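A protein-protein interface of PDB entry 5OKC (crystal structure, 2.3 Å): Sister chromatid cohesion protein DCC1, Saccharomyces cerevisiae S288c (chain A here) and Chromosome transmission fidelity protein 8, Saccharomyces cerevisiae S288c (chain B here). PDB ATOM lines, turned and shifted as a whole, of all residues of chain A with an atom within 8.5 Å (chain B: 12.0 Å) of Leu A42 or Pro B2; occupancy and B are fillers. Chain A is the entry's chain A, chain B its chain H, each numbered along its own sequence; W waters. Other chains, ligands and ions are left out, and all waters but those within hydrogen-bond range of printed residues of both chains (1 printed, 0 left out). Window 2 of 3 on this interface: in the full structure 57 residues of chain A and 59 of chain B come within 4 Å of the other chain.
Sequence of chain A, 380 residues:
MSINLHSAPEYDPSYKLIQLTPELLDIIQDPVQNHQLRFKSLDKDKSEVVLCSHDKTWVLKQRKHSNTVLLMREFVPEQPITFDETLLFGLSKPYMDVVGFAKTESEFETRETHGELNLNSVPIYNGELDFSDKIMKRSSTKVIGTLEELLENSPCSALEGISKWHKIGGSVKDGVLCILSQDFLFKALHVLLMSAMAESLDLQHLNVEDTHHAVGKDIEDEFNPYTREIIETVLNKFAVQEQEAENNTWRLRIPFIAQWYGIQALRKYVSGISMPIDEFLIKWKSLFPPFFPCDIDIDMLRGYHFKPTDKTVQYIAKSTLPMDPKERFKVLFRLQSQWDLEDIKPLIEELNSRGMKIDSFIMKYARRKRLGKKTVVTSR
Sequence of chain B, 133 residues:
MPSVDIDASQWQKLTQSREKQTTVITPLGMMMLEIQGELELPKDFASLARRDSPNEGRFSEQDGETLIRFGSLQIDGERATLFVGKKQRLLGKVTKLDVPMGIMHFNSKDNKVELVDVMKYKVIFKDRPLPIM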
ATOM      1  N   ARG A  38      -0.285 -22.511   1.033  1.00  0.00           N
ATOM      2  CA  ARG A  38       0.558 -23.632   1.421  1.00  0.00           C
ATOM      3  C   ARG A  38       1.835 -23.176   2.114  1.00  0.00           C
ATOM      4  O   ARG A  38       2.517 -22.278   1.633  1.00  0.00           O
ATOM      5  CB  ARG A  38       0.897 -24.462   0.180  1.00  0.00           C
ATOM      6  CG  ARG A  38       1.647 -25.747   0.450  1.00  0.00           C
ATOM      7  CD  ARG A  38       1.792 -26.556  -0.833  1.00  0.00           C
ATOM      8  NE  ARG A  38       2.433 -27.848  -0.598  1.00  0.00           N
ATOM      9  CZ  ARG A  38       1.778 -28.980  -0.369  1.00  0.00           C
ATOM     10  NH1 ARG A  38       2.447 -30.107  -0.166  1.00  0.00           N
ATOM     11  NH2 ARG A  38       0.452 -28.991  -0.343  1.00  0.00           N
ATOM     12  N   PHE A  39       2.161 -23.794   3.246  1.00  0.00           N
ATOM     13  CA  PHE A  39       3.446 -23.540   3.892  1.00  0.00           C
ATOM     14  C   PHE A  39       4.518 -24.432   3.271  1.00  0.00           C
ATOM     15  O   PHE A  39       4.326 -25.640   3.135  1.00  0.00           O
ATOM     16  CB  PHE A  39       3.366 -23.775   5.402  1.00  0.00           C
ATOM     17  CG  PHE A  39       2.544 -22.749   6.134  1.00  0.00           C
ATOM     18  CD1 PHE A  39       3.025 -21.463   6.324  1.00  0.00           C
ATOM     19  CD2 PHE A  39       1.302 -23.077   6.652  1.00  0.00           C
ATOM     20  CE1 PHE A  39       2.274 -20.520   7.002  1.00  0.00           C
ATOM     21  CE2 PHE A  39       0.548 -22.138   7.336  1.00  0.00           C
ATOM     22  CZ  PHE A  39       1.034 -20.859   7.509  1.00  0.00           C
ATOM     23  N   LYS A  40       5.644 -23.833   2.895  1.00  0.00           N
ATOM     24  CA  LYS A  40       6.729 -24.569   2.251  1.00  0.00           C
ATOM     25  C   LYS A  40       8.072 -24.290   2.911  1.00  0.00           C
ATOM     26  O   LYS A  40       8.345 -23.170   3.339  1.00  0.00           O
ATOM     27  CB  LYS A  40       6.809 -24.215   0.763  1.00  0.00           C
ATOM     28  CG  LYS A  40       5.616 -24.665  -0.060  1.00  0.00           C
ATOM     29  CD  LYS A  40       5.754 -24.228  -1.511  1.00  0.00           C
ATOM     30  CE  LYS A  40       6.987 -24.840  -2.156  1.00  0.00           C
ATOM     31  NZ  LYS A  40       7.123 -24.447  -3.584  1.00  0.00           N
ATOM     32  N   SER A  41       8.911 -25.319   2.985  1.00  0.00           N
ATOM     33  CA  SER A  41      10.254 -25.179   3.529  1.00  0.00           C
ATOM     34  C   SER A  41      11.172 -26.255   2.959  1.00  0.00           C
ATOM     35  O   SER A  41      10.723 -27.353   2.635  1.00  0.00           O
ATOM     36  CB  SER A  41      10.230 -25.255   5.056  1.00  0.00           C
ATOM     37  OG  SER A  41      11.518 -25.023   5.596  1.00  0.00           O
ATOM     38  N   LEU A  42      12.455 -25.933   2.829  1.00  0.00           N
ATOM     39  CA  LEU A  42      13.425 -26.889   2.306  1.00  0.00           C
ATOM     40  C   LEU A  42      13.668 -28.007   3.314  1.00  0.00           C
ATOM     41  O   LEU A  42      13.800 -29.174   2.944  1.00  0.00           O
ATOM     42  CB  LEU A  42      14.742 -26.190   1.962  1.00  0.00           C
ATOM     43  CG  LEU A  42      15.869 -27.090   1.450  1.00  0.00           C
ATOM     44  CD1 LEU A  42      15.443 -27.805   0.177  1.00  0.00           C
ATOM     45  CD2 LEU A  42      17.138 -26.286   1.217  1.00  0.00           C
ATOM     46  N   ASP A  43      13.720 -27.639   4.591  1.00  0.00           N
ATOM     47  CA  ASP A  43      13.920 -28.598   5.671  1.00  0.00           C
ATOM     48  C   ASP A  43      13.136 -28.165   6.904  1.00  0.00           C
ATOM     49  O   ASP A  43      12.444 -27.148   6.877  1.00  0.00           O
ATOM     50  CB  ASP A  43      15.410 -28.744   5.998  1.00  0.00           C
ATOM     51  CG  ASP A  43      16.095 -27.410   6.235  1.00  0.00           C
ATOM     52  OD1 ASP A  43      15.668 -26.665   7.142  1.00  0.00           O
ATOM     53  OD2 ASP A  43      17.064 -27.105   5.508  1.00  0.00           O
ATOM     54  N   LYS A  44      13.237 -28.935   7.981  1.00  0.00           N
ATOM     55  CA  LYS A  44      12.433 -28.667   9.170  1.00  0.00           C
ATOM     56  C   LYS A  44      13.128 -27.811  10.231  1.00  0.00           C
ATOM     57  O   LYS A  44      12.462 -27.105  10.987  1.00  0.00           O
ATOM     58  CB  LYS A  44      11.960 -29.978   9.807  1.00  0.00           C
ATOM     59  CG  LYS A  44      10.976 -30.759   8.950  1.00  0.00           C
ATOM     60  CD  LYS A  44      10.330 -31.887   9.739  1.00  0.00           C
ATOM     61  CE  LYS A  44       9.290 -32.620   8.906  1.00  0.00           C
ATOM     62  NZ  LYS A  44       8.643 -33.727   9.665  1.00  0.00           N
ATOM     63  N   ASP A  45      14.454 -27.870  10.292  1.00  0.00           N
ATOM     64  CA  ASP A  45      15.173 -27.277  11.418  1.00  0.00           C
ATOM     65  C   ASP A  45      15.953 -26.002  11.090  1.00  0.00           C
ATOM     66  O   ASP A  45      16.269 -25.224  11.989  1.00  0.00           O
ATOM     67  CB  ASP A  45      16.136 -28.307  12.012  1.00  0.00           C
ATOM     68  CG  ASP A  45      17.120 -28.840  10.990  1.00  0.00           C
ATOM     69  OD1 ASP A  45      16.804 -28.793   9.781  1.00  0.00           O
ATOM     70  OD2 ASP A  45      18.208 -29.302  11.391  1.00  0.00           O
ATOM     71  N   LYS A  46      16.265 -25.783   9.817  1.00  0.00           N
ATOM     72  CA  LYS A  46      17.157 -24.686   9.449  1.00  0.00           C
ATOM     73  C   LYS A  46      16.509 -23.645   8.539  1.00  0.00           C
ATOM     74  O   LYS A  46      16.520 -22.452   8.841  1.00  0.00           O
ATOM     75  CB  LYS A  46      18.412 -25.236   8.766  1.00  0.00           C
ATOM     76  CG  LYS A  46      19.108 -26.355   9.524  1.00  0.00           C
ATOM     77  CD  LYS A  46      19.809 -25.837  10.770  1.00  0.00           C
ATOM     78  CE  LYS A  46      20.622 -26.934  11.442  1.00  0.00           C
ATOM     79  NZ  LYS A  46      21.378 -26.429  12.622  1.00  0.00           N
ATOM     80  N   SER A  47      15.945 -24.101   7.427  1.00  0.00           N
ATOM     81  CA  SER A  47      15.495 -23.199   6.373  1.00  0.00           C
ATOM     82  C   SER A  47      14.236 -22.421   6.738  1.00  0.00           C
ATOM     83  O   SER A  47      13.482 -22.813   7.629  1.00  0.00           O
ATOM     84  CB  SER A  47      15.251 -23.986   5.082  1.00  0.00           C
ATOM     85  OG  SER A  47      14.257 -24.978   5.274  1.00  0.00           O
ATOM     86  N   GLU A  48      14.023 -21.310   6.038  1.00  0.00           N
ATOM     87  CA  GLU A  48      12.848 -20.472   6.243  1.00  0.00           C
ATOM     88  C   GLU A  48      11.585 -21.177   5.766  1.00  0.00           C
ATOM     89  O   GLU A  48      11.643 -22.069   4.916  1.00  0.00           O
ATOM     90  CB  GLU A  48      12.999 -19.140   5.503  1.00  0.00           C
ATOM     91  CG  GLU A  48      12.860 -19.267   3.988  1.00  0.00           C
ATOM     92  CD  GLU A  48      13.031 -17.947   3.259  1.00  0.00           C
ATOM     93  OE1 GLU A  48      12.568 -16.910   3.778  1.00  0.00           O
ATOM     94  OE2 GLU A  48      13.627 -17.949   2.159  1.00  0.00           O
ATOM     95  N   VAL A  49      10.445 -20.782   6.319  1.00  0.00           N
ATOM     96  CA  VAL A  49       9.166 -21.257   5.816  1.00  0.00           C
ATOM     97  C   VAL A  49       8.458 -20.101   5.118  1.00  0.00           C
ATOM     98  O   VAL A  49       8.422 -18.982   5.629  1.00  0.00           O
ATOM     99  CB  VAL A  49       8.275 -21.845   6.936  1.00  0.00           C
ATOM    100  CG1 VAL A  49       8.083 -20.848   8.060  1.00  0.00           C
ATOM    101  CG2 VAL A  49       6.932 -22.290   6.375  1.00  0.00           C
ATOM    102  N   VAL A  50       7.928 -20.368   3.930  1.00  0.00           N
ATOM    103  CA  VAL A  50       7.192 -19.362   3.178  1.00  0.00           C
ATOM    104  C   VAL A  50       5.737 -19.780   2.996  1.00  0.00           C
ATOM    105  O   VAL A  50       5.397 -20.957   3.114  1.00  0.00           O
ATOM    106  CB  VAL A  50       7.827 -19.109   1.797  1.00  0.00           C
ATOM    107  CG1 VAL A  50       9.226 -18.538   1.957  1.00  0.00           C
ATOM    108  CG2 VAL A  50       7.861 -20.391   0.980  1.00  0.00           C
ATOM    109  N   ASN A 118      15.523 -22.594  -5.801  1.00  0.00           N
ATOM    110  CA  ASN A 118      16.664 -23.126  -5.072  1.00  0.00           C
ATOM    111  C   ASN A 118      17.607 -23.815  -6.046  1.00  0.00           C
ATOM    112  O   ASN A 118      17.414 -24.979  -6.394  1.00  0.00           O
ATOM    113  CB  ASN A 118      16.203 -24.099  -3.985  1.00  0.00           C
ATOM    114  CG  ASN A 118      17.361 -24.760  -3.259  1.00  0.00           C
ATOM    115  OD1 ASN A 118      18.470 -24.227  -3.212  1.00  0.00           O
ATOM    116  ND2 ASN A 118      17.104 -25.929  -2.684  1.00  0.00           N
ATOM    117  N   LEU A 119      18.633 -23.091  -6.480  1.00  0.00           N
ATOM    118  CA  LEU A 119      19.527 -23.600  -7.510  1.00  0.00           C
ATOM    119  C   LEU A 119      20.826 -24.146  -6.928  1.00  0.00           C
ATOM    120  O   LEU A 119      21.898 -23.966  -7.505  1.00  0.00           O
ATOM    121  CB  LEU A 119      19.833 -22.510  -8.540  1.00  0.00           C
ATOM    122  CG  LEU A 119      18.625 -21.907  -9.263  1.00  0.00           C
ATOM    123  CD1 LEU A 119      19.059 -20.787 -10.196  1.00  0.00           C
ATOM    124  CD2 LEU A 119      17.857 -22.978 -10.022  1.00  0.00           C
ATOM    125  N   ASN A 120      20.718 -24.810  -5.784  1.00  0.00           N
ATOM    126  CA  ASN A 120      21.880 -25.342  -5.085  1.00  0.00           C
ATOM    127  C   ASN A 120      22.601 -26.426  -5.894  1.00  0.00           C
ATOM    128  O   ASN A 120      23.772 -26.271  -6.244  1.00  0.00           O
ATOM    129  CB  ASN A 120      21.459 -25.887  -3.715  1.00  0.00           C
ATOM    130  CG  ASN A 120      22.643 -26.284  -2.838  1.00  0.00           C
ATOM    131  OD1 ASN A 120      23.780 -26.391  -3.298  1.00  0.00           O
ATOM    132  ND2 ASN A 120      22.369 -26.504  -1.557  1.00  0.00           N
ATOM    133  N   ILE A 144      19.018 -33.166  -8.759  1.00  0.00           N
ATOM    134  CA  ILE A 144      17.601 -32.879  -8.955  1.00  0.00           C
ATOM    135  C   ILE A 144      17.140 -33.513 -10.263  1.00  0.00           C
ATOM    136  O   ILE A 144      17.550 -33.098 -11.346  1.00  0.00           O
ATOM    137  CB  ILE A 144      17.310 -31.368  -8.977  1.00  0.00           C
ATOM    138  CG1 ILE A 144      17.701 -30.734  -7.643  1.00  0.00           C
ATOM    139  CG2 ILE A 144      15.837 -31.120  -9.245  1.00  0.00           C
ATOM    140  CD1 ILE A 144      16.999 -31.346  -6.449  1.00  0.00           C
ATOM    141  N   GLU A 149      10.329 -31.483  -8.628  1.00  0.00           N
ATOM    142  CA  GLU A 149      11.135 -31.615  -7.420  1.00  0.00           C
ATOM    143  C   GLU A 149      11.823 -30.299  -7.079  1.00  0.00           C
ATOM    144  O   GLU A 149      11.904 -29.914  -5.912  1.00  0.00           O
ATOM    145  CB  GLU A 149      12.177 -32.723  -7.592  1.00  0.00           C
ATOM    146  CG  GLU A 149      13.142 -32.861  -6.425  1.00  0.00           C
ATOM    147  CD  GLU A 149      14.250 -33.860  -6.700  1.00  0.00           C
ATOM    148  OE1 GLU A 149      15.048 -34.135  -5.779  1.00  0.00           O
ATOM    149  OE2 GLU A 149      14.325 -34.366  -7.840  1.00  0.00           O
ATOM    150  N   LEU A 150      12.314 -29.613  -8.106  1.00  0.00           N
ATOM    151  CA  LEU A 150      12.969 -28.324  -7.924  1.00  0.00           C
ATOM    152  C   LEU A 150      12.014 -27.288  -7.337  1.00  0.00           C
ATOM    153  O   LEU A 150      12.342 -26.611  -6.364  1.00  0.00           O
ATOM    154  CB  LEU A 150      13.535 -27.819  -9.250  1.00  0.00           C
ATOM    155  CG  LEU A 150      14.362 -26.537  -9.150  1.00  0.00           C
ATOM    156  CD1 LEU A 150      15.626 -26.788  -8.350  1.00  0.00           C
ATOM    157  CD2 LEU A 150      14.692 -25.996 -10.531  1.00  0.00           C
ATOM    158  N   GLU A 152       9.250 -27.895  -5.805  1.00  0.00           N
ATOM    159  CA  GLU A 152       8.813 -28.384  -4.504  1.00  0.00           C
ATOM    160  C   GLU A 152       9.791 -27.989  -3.401  1.00  0.00           C
ATOM    161  O   GLU A 152       9.384 -27.653  -2.289  1.00  0.00           O
ATOM    162  CB  GLU A 152       8.647 -29.906  -4.539  1.00  0.00           C
ATOM    163  CG  GLU A 152       8.178 -30.517  -3.228  1.00  0.00           C
ATOM    164  CD  GLU A 152       6.802 -30.028  -2.815  1.00  0.00           C
ATOM    165  OE1 GLU A 152       6.003 -29.660  -3.702  1.00  0.00           O
ATOM    166  OE2 GLU A 152       6.518 -30.008  -1.598  1.00  0.00           O
ATOM    167  N   ASN A 153      11.081 -28.026  -3.718  1.00  0.00           N
ATOM    168  CA  ASN A 153      12.118 -27.695  -2.748  1.00  0.00           C
ATOM    169  C   ASN A 153      12.659 -26.277  -2.912  1.00  0.00           C
ATOM    170  O   ASN A 153      13.802 -25.996  -2.549  1.00  0.00           O
ATOM    171  CB  ASN A 153      13.265 -28.700  -2.842  1.00  0.00           C
ATOM    172  CG  ASN A 153      12.843 -30.101  -2.445  1.00  0.00           C
ATOM    173  OD1 ASN A 153      12.762 -30.424  -1.259  1.00  0.00           O
ATOM    174  ND2 ASN A 153      12.569 -30.941  -3.436  1.00  0.00           N
ATOM    175  N   SER A 154      11.835 -25.388  -3.457  1.00  0.00           N
ATOM    176  CA  SER A 154      12.224 -23.992  -3.633  1.00  0.00           C
ATOM    177  C   SER A 154      11.272 -23.063  -2.885  1.00  0.00           C
ATOM    178  O   SER A 154      10.080 -23.353  -2.768  1.00  0.00           O
ATOM    179  CB  SER A 154      12.259 -23.624  -5.118  1.00  0.00           C
ATOM    180  OG  SER A 154      13.288 -24.327  -5.795  1.00  0.00           O
ATOM    181  N   PRO A 155      11.798 -21.940  -2.373  1.00  0.00           N
ATOM    182  CA  PRO A 155      10.970 -20.933  -1.703  1.00  0.00           C
ATOM    183  C   PRO A 155      10.250 -20.028  -2.699  1.00  0.00           C
ATOM    184  O   PRO A 155      10.564 -18.841  -2.797  1.00  0.00           O
ATOM    185  CB  PRO A 155      11.987 -20.141  -0.882  1.00  0.00           C
ATOM    186  CG  PRO A 155      13.244 -20.238  -1.678  1.00  0.00           C
ATOM    187  CD  PRO A 155      13.232 -21.610  -2.301  1.00  0.00           C
ATOM    188  N   PRO B   2       9.710 -29.874   3.619  1.00  0.00           N
ATOM    189  CA  PRO B   2       8.320 -30.314   3.776  1.00  0.00           C
ATOM    190  C   PRO B   2       7.325 -29.262   3.301  1.00  0.00           C
ATOM    191  O   PRO B   2       7.705 -28.115   3.064  1.00  0.00           O
ATOM    192  CB  PRO B   2       8.195 -30.545   5.284  1.00  0.00           C
ATOM    193  CG  PRO B   2       9.205 -29.631   5.881  1.00  0.00           C
ATOM    194  CD  PRO B   2      10.356 -29.618   4.918  1.00  0.00           C
ATOM    195  N   SER B   3       6.063 -29.653   3.172  1.00  0.00           N
ATOM    196  CA  SER B   3       5.033 -28.744   2.691  1.00  0.00           C
ATOM    197  C   SER B   3       3.634 -29.242   3.049  1.00  0.00           C
ATOM    198  O   SER B   3       3.393 -30.447   3.102  1.00  0.00           O
ATOM    199  CB  SER B   3       5.159 -28.568   1.178  1.00  0.00           C
ATOM    200  OG  SER B   3       4.339 -27.514   0.722  1.00  0.00           O
ATOM    201  N   VAL B   4       2.715 -28.308   3.290  1.00  0.00           N
ATOM    202  CA  VAL B   4       1.343 -28.662   3.646  1.00  0.00           C
ATOM    203  C   VAL B   4       0.372 -27.509   3.368  1.00  0.00           C
ATOM    204  O   VAL B   4       0.686 -26.341   3.604  1.00  0.00           O
ATOM    205  CB  VAL B   4       1.239 -29.078   5.132  1.00  0.00           C
ATOM    206  CG1 VAL B   4       1.708 -27.953   6.039  1.00  0.00           C
ATOM    207  CG2 VAL B   4      -0.183 -29.504   5.482  1.00  0.00           C
ATOM    208  N   ASP B   5      -0.808 -27.846   2.857  1.00  0.00           N
ATOM    209  CA  ASP B   5      -1.833 -26.851   2.570  1.00  0.00           C
ATOM    210  C   ASP B   5      -2.521 -26.364   3.840  1.00  0.00           C
ATOM    211  O   ASP B   5      -2.591 -27.084   4.836  1.00  0.00           O
ATOM    212  CB  ASP B   5      -2.879 -27.423   1.610  1.00  0.00           C
ATOM    213  CG  ASP B   5      -2.309 -27.723   0.239  1.00  0.00           C
ATOM    214  OD1 ASP B   5      -1.317 -27.073  -0.148  1.00  0.00           O
ATOM    215  OD2 ASP B   5      -2.855 -28.609  -0.451  1.00  0.00           O
ATOM    216  N   ILE B   6      -3.024 -25.134   3.796  1.00  0.00           N
ATOM    217  CA  ILE B   6      -3.850 -24.607   4.872  1.00  0.00           C
ATOM    218  C   ILE B   6      -5.303 -25.005   4.648  1.00  0.00           C
ATOM    219  O   ILE B   6      -5.886 -24.685   3.613  1.00  0.00           O
ATOM    220  CB  ILE B   6      -3.757 -23.075   4.969  1.00  0.00           C
ATOM    221  CG1 ILE B   6      -2.332 -22.641   5.313  1.00  0.00           C
ATOM    222  CG2 ILE B   6      -4.738 -22.550   6.005  1.00  0.00           C
ATOM    223  CD1 ILE B   6      -2.160 -21.140   5.363  1.00  0.00           C
ATOM    224  N   PHE B 106      -1.980 -25.619  14.461  1.00  0.00           N
ATOM    225  CA  PHE B 106      -0.931 -26.436  13.873  1.00  0.00           C
ATOM    226  C   PHE B 106      -0.890 -27.821  14.506  1.00  0.00           C
ATOM    227  O   PHE B 106      -0.359 -28.003  15.602  1.00  0.00           O
ATOM    228  CB  PHE B 106       0.424 -25.741  14.009  1.00  0.00           C
ATOM    229  CG  PHE B 106       0.561 -24.515  13.152  1.00  0.00           C
ATOM    230  CD1 PHE B 106       0.054 -23.296  13.570  1.00  0.00           C
ATOM    231  CD2 PHE B 106       1.196 -24.583  11.921  1.00  0.00           C
ATOM    232  CE1 PHE B 106       0.178 -22.168  12.780  1.00  0.00           C
ATOM    233  CE2 PHE B 106       1.325 -23.459  11.125  1.00  0.00           C
ATOM    234  CZ  PHE B 106       0.815 -22.250  11.555  1.00  0.00           C
ATOM    235  N   ASN B 107      -1.464 -28.793  13.802  1.00  0.00           N
ATOM    236  CA  ASN B 107      -1.481 -30.177  14.256  1.00  0.00           C
ATOM    237  C   ASN B 107      -0.131 -30.842  14.028  1.00  0.00           C
ATOM    238  O   ASN B 107       0.166 -31.281  12.920  1.00  0.00           O
ATOM    239  CB  ASN B 107      -2.580 -30.961  13.536  1.00  0.00           C
ATOM    240  CG  ASN B 107      -2.708 -32.386  14.039  1.00  0.00           C
ATOM    241  OD1 ASN B 107      -2.249 -32.716  15.133  1.00  0.00           O
ATOM    242  ND2 ASN B 107      -3.328 -33.243  13.236  1.00  0.00           N
ATOM    243  N   SER B 108       0.680 -30.912  15.079  1.00  0.00           N
ATOM    244  CA  SER B 108       2.032 -31.444  14.963  1.00  0.00           C
ATOM    245  C   SER B 108       2.027 -32.905  14.530  1.00  0.00           C
ATOM    246  O   SER B 108       2.890 -33.327  13.765  1.00  0.00           O
ATOM    247  CB  SER B 108       2.780 -31.299  16.291  1.00  0.00           C
ATOM    248  OG  SER B 108       3.140 -29.949  16.529  1.00  0.00           O
ATOM    249  N   LYS B 109       1.044 -33.662  15.008  1.00  0.00           N
ATOM    250  CA  LYS B 109       0.936 -35.089  14.707  1.00  0.00           C
ATOM    251  C   LYS B 109       0.955 -35.382  13.207  1.00  0.00           C
ATOM    252  O   LYS B 109       1.770 -36.173  12.732  1.00  0.00           O
ATOM    253  CB  LYS B 109      -0.338 -35.664  15.326  1.00  0.00           C
ATOM    254  CG  LYS B 109      -0.663 -37.077  14.869  1.00  0.00           C
ATOM    255  CD  LYS B 109      -2.057 -37.495  15.307  1.00  0.00           C
ATOM    256  CE  LYS B 109      -2.394 -38.889  14.803  1.00  0.00           C
ATOM    257  NZ  LYS B 109      -3.760 -39.314  15.213  1.00  0.00           N
ATOM    258  N   ASP B 110       0.054 -34.742  12.466  1.00  0.00           N
ATOM    259  CA  ASP B 110      -0.064 -34.975  11.031  1.00  0.00           C
ATOM    260  C   ASP B 110       0.544 -33.845  10.203  1.00  0.00           C
ATOM    261  O   ASP B 110       0.446 -33.855   8.975  1.00  0.00           O
ATOM    262  CB  ASP B 110      -1.532 -35.162  10.643  1.00  0.00           C
ATOM    263  CG  ASP B 110      -2.202 -36.278  11.420  1.00  0.00           C
ATOM    264  OD1 ASP B 110      -1.545 -37.313  11.662  1.00  0.00           O
ATOM    265  OD2 ASP B 110      -3.385 -36.118  11.791  1.00  0.00           O
ATOM    266  N   ASN B 111       1.169 -32.883  10.880  1.00  0.00           N
ATOM    267  CA  ASN B 111       1.707 -31.684  10.232  1.00  0.00           C
ATOM    268  C   ASN B 111       0.675 -30.991   9.347  1.00  0.00           C
ATOM    269  O   ASN B 111       0.971 -30.609   8.216  1.00  0.00           O
ATOM    270  CB  ASN B 111       2.953 -32.029   9.413  1.00  0.00           C
ATOM    271  CG  ASN B 111       4.225 -31.988  10.240  1.00  0.00           C
ATOM    272  OD1 ASN B 111       5.260 -31.501   9.784  1.00  0.00           O
ATOM    273  ND2 ASN B 111       4.150 -32.488  11.469  1.00  0.00           N
ATOM    274  N   LYS B 112      -0.535 -30.835   9.874  1.00  0.00           N
ATOM    275  CA  LYS B 112      -1.619 -30.182   9.148  1.00  0.00           C
ATOM    276  C   LYS B 112      -2.008 -28.860   9.800  1.00  0.00           C
ATOM    277  O   LYS B 112      -1.969 -28.728  11.022  1.00  0.00           O
ATOM    278  CB  LYS B 112      -2.837 -31.105   9.059  1.00  0.00           C
ATOM    279  CG  LYS B 112      -2.598 -32.358   8.229  1.00  0.00           C
ATOM    280  CD  LYS B 112      -3.889 -33.120   7.968  1.00  0.00           C
ATOM    281  CE  LYS B 112      -4.559 -33.547   9.263  1.00  0.00           C
ATOM    282  NZ  LYS B 112      -5.804 -34.322   9.006  1.00  0.00           N
ATOM    283  N   VAL B 113      -2.376 -27.883   8.976  1.00  0.00           N
ATOM    284  CA  VAL B 113      -2.808 -26.583   9.473  1.00  0.00           C
ATOM    285  C   VAL B 113      -4.276 -26.345   9.164  1.00  0.00           C
ATOM    286  O   VAL B 113      -4.730 -26.556   8.039  1.00  0.00           O
ATOM    287  CB  VAL B 113      -2.000 -25.425   8.857  1.00  0.00           C
ATOM    288  CG1 VAL B 113      -2.255 -24.140   9.626  1.00  0.00           C
ATOM    289  CG2 VAL B 113      -0.537 -25.745   8.856  1.00  0.00           C
HETATM  290  O   HOH W   1       4.636 -27.902  -2.314  1.00  0.00           O
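N of Ser A41 is in hydrogen-bond range of O of Pro B2. O of Phe A39 sits at hydrogen-bond distance from OG of Ser B3, 3.1 Å away. The backbone NH (N) of Phe A39 sits at hydrogen-bond distance from the backbone carbonyl oxygen (O) of Val B4, at 3.0 Å. NH1 of Arg A38 lies close to OG of Ser B3 (3.3 Å). The guanidinium group of Arg A38 lies within salt-bridge range of the side-chain carboxylate of Asp B5, at 2.6 Å.
The backbone NH (N) of Ser A47 sits at hydrogen-bond distance from the side-chain carboxylate (OD1) of Asp A43. The side-chain hydroxyl of Ser A41 lies within hydrogen-bond range of the side-chain hydroxyl of Ser A47 (2.8 Å). The side-chain hydroxyl of Ser A41 sits at hydrogen-bond distance from the backbone carbonyl oxygen of Asp A43, 2.6 Å away. The backbone carbonyl oxygen of Glu A48 is in hydrogen-bond range of the side-chain hydroxyl of Ser A41. The backbone NH of Val A50 lies within hydrogen-bond range of the backbone carbonyl oxygen of Lys A40 (2.9 Å). O of Ser A154 sits at hydrogen-bond distance from NZ of Lys A40 (3.3 Å).
Arg A38 touches Val B4. Ile B6 touches Phe A39 (CD1 to CE2, 3.5 Å). Phe A39 touches Val B113. CA of Lys A40 touches O of Pro B2, 3.8 Å away. CG of Lys A40 touches OG of Ser B3, at 3.2 Å. Leu A42 touches Pro B2. Pro B2 touches Asp A43. Pro B2 touches Lys A44 (CG to CG, 3.7 Å). CB of Ser B3 touches OE2 of Glu A152, at 3.4 Å.
Of the printed residues of chain B, Leu A42 touches Pro B2 (3.99 Å). Lys A40 touches just these residues of chain B: Pro B2 and Ser B3. Of chain B, only Pro B2 comes within 4 Å of Ser A41. Asp A43 touches just one residue of chain B: Pro B2. Lys A44 touches just one residue of chain B: Pro B2. No residue of chain B comes within 4 Å of Ser A47. No residue of chain B comes within 4 Å of Asn A118. Ser B3 touches four residues of chain A. Of the printed residues of chain A, Val B4 touches Arg A38 and Phe A39. Of the printed residues of chain B, Phe A39 touches Ser B3, Val B4, Ile B6 and Val B113. Of the printed residues of chain A, Asp B5 touches Arg A38 (2.6 Å). Printed residues of chain B within 4 Å of Arg A38: Ser B3 (2.3 Å), Val B4 (3.4 Å) and Asp B5 (2.6 Å). Printed residues of chain A within 4 Å of Ile B6: Phe A39 (3.5 Å). Asn A120 touches none of the printed residues of chain B. Leu A150 touches none of the printed residues of chain B. The nearest printed residue of chain B that does not touch Leu A42 is Ser B3 (7.4 Å). The nearest printed residue of chain A that does not touch Val B4 is Lys A40 (5.4 Å).
Printed residues of chain B that touch a printed residue of chain A: Pro B2, Ser B3, Val B4, Asp B5, Ile B6 and Val B113. Hydrophobic or aromatic side chains of chain B within 4 Å of the printed part of chain A: Pro B2, Ile B6 and Val B113. Among the printed residues, Asp or Glu carboxylates within 4 Å of a Lys or Arg side-chain nitrogen of the other chain: Arg A38 with Asp B5.
Water W1 lies within hydrogen-bond range of OE1 of Glu A152, NE of Arg A38 and OG of Ser B3.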
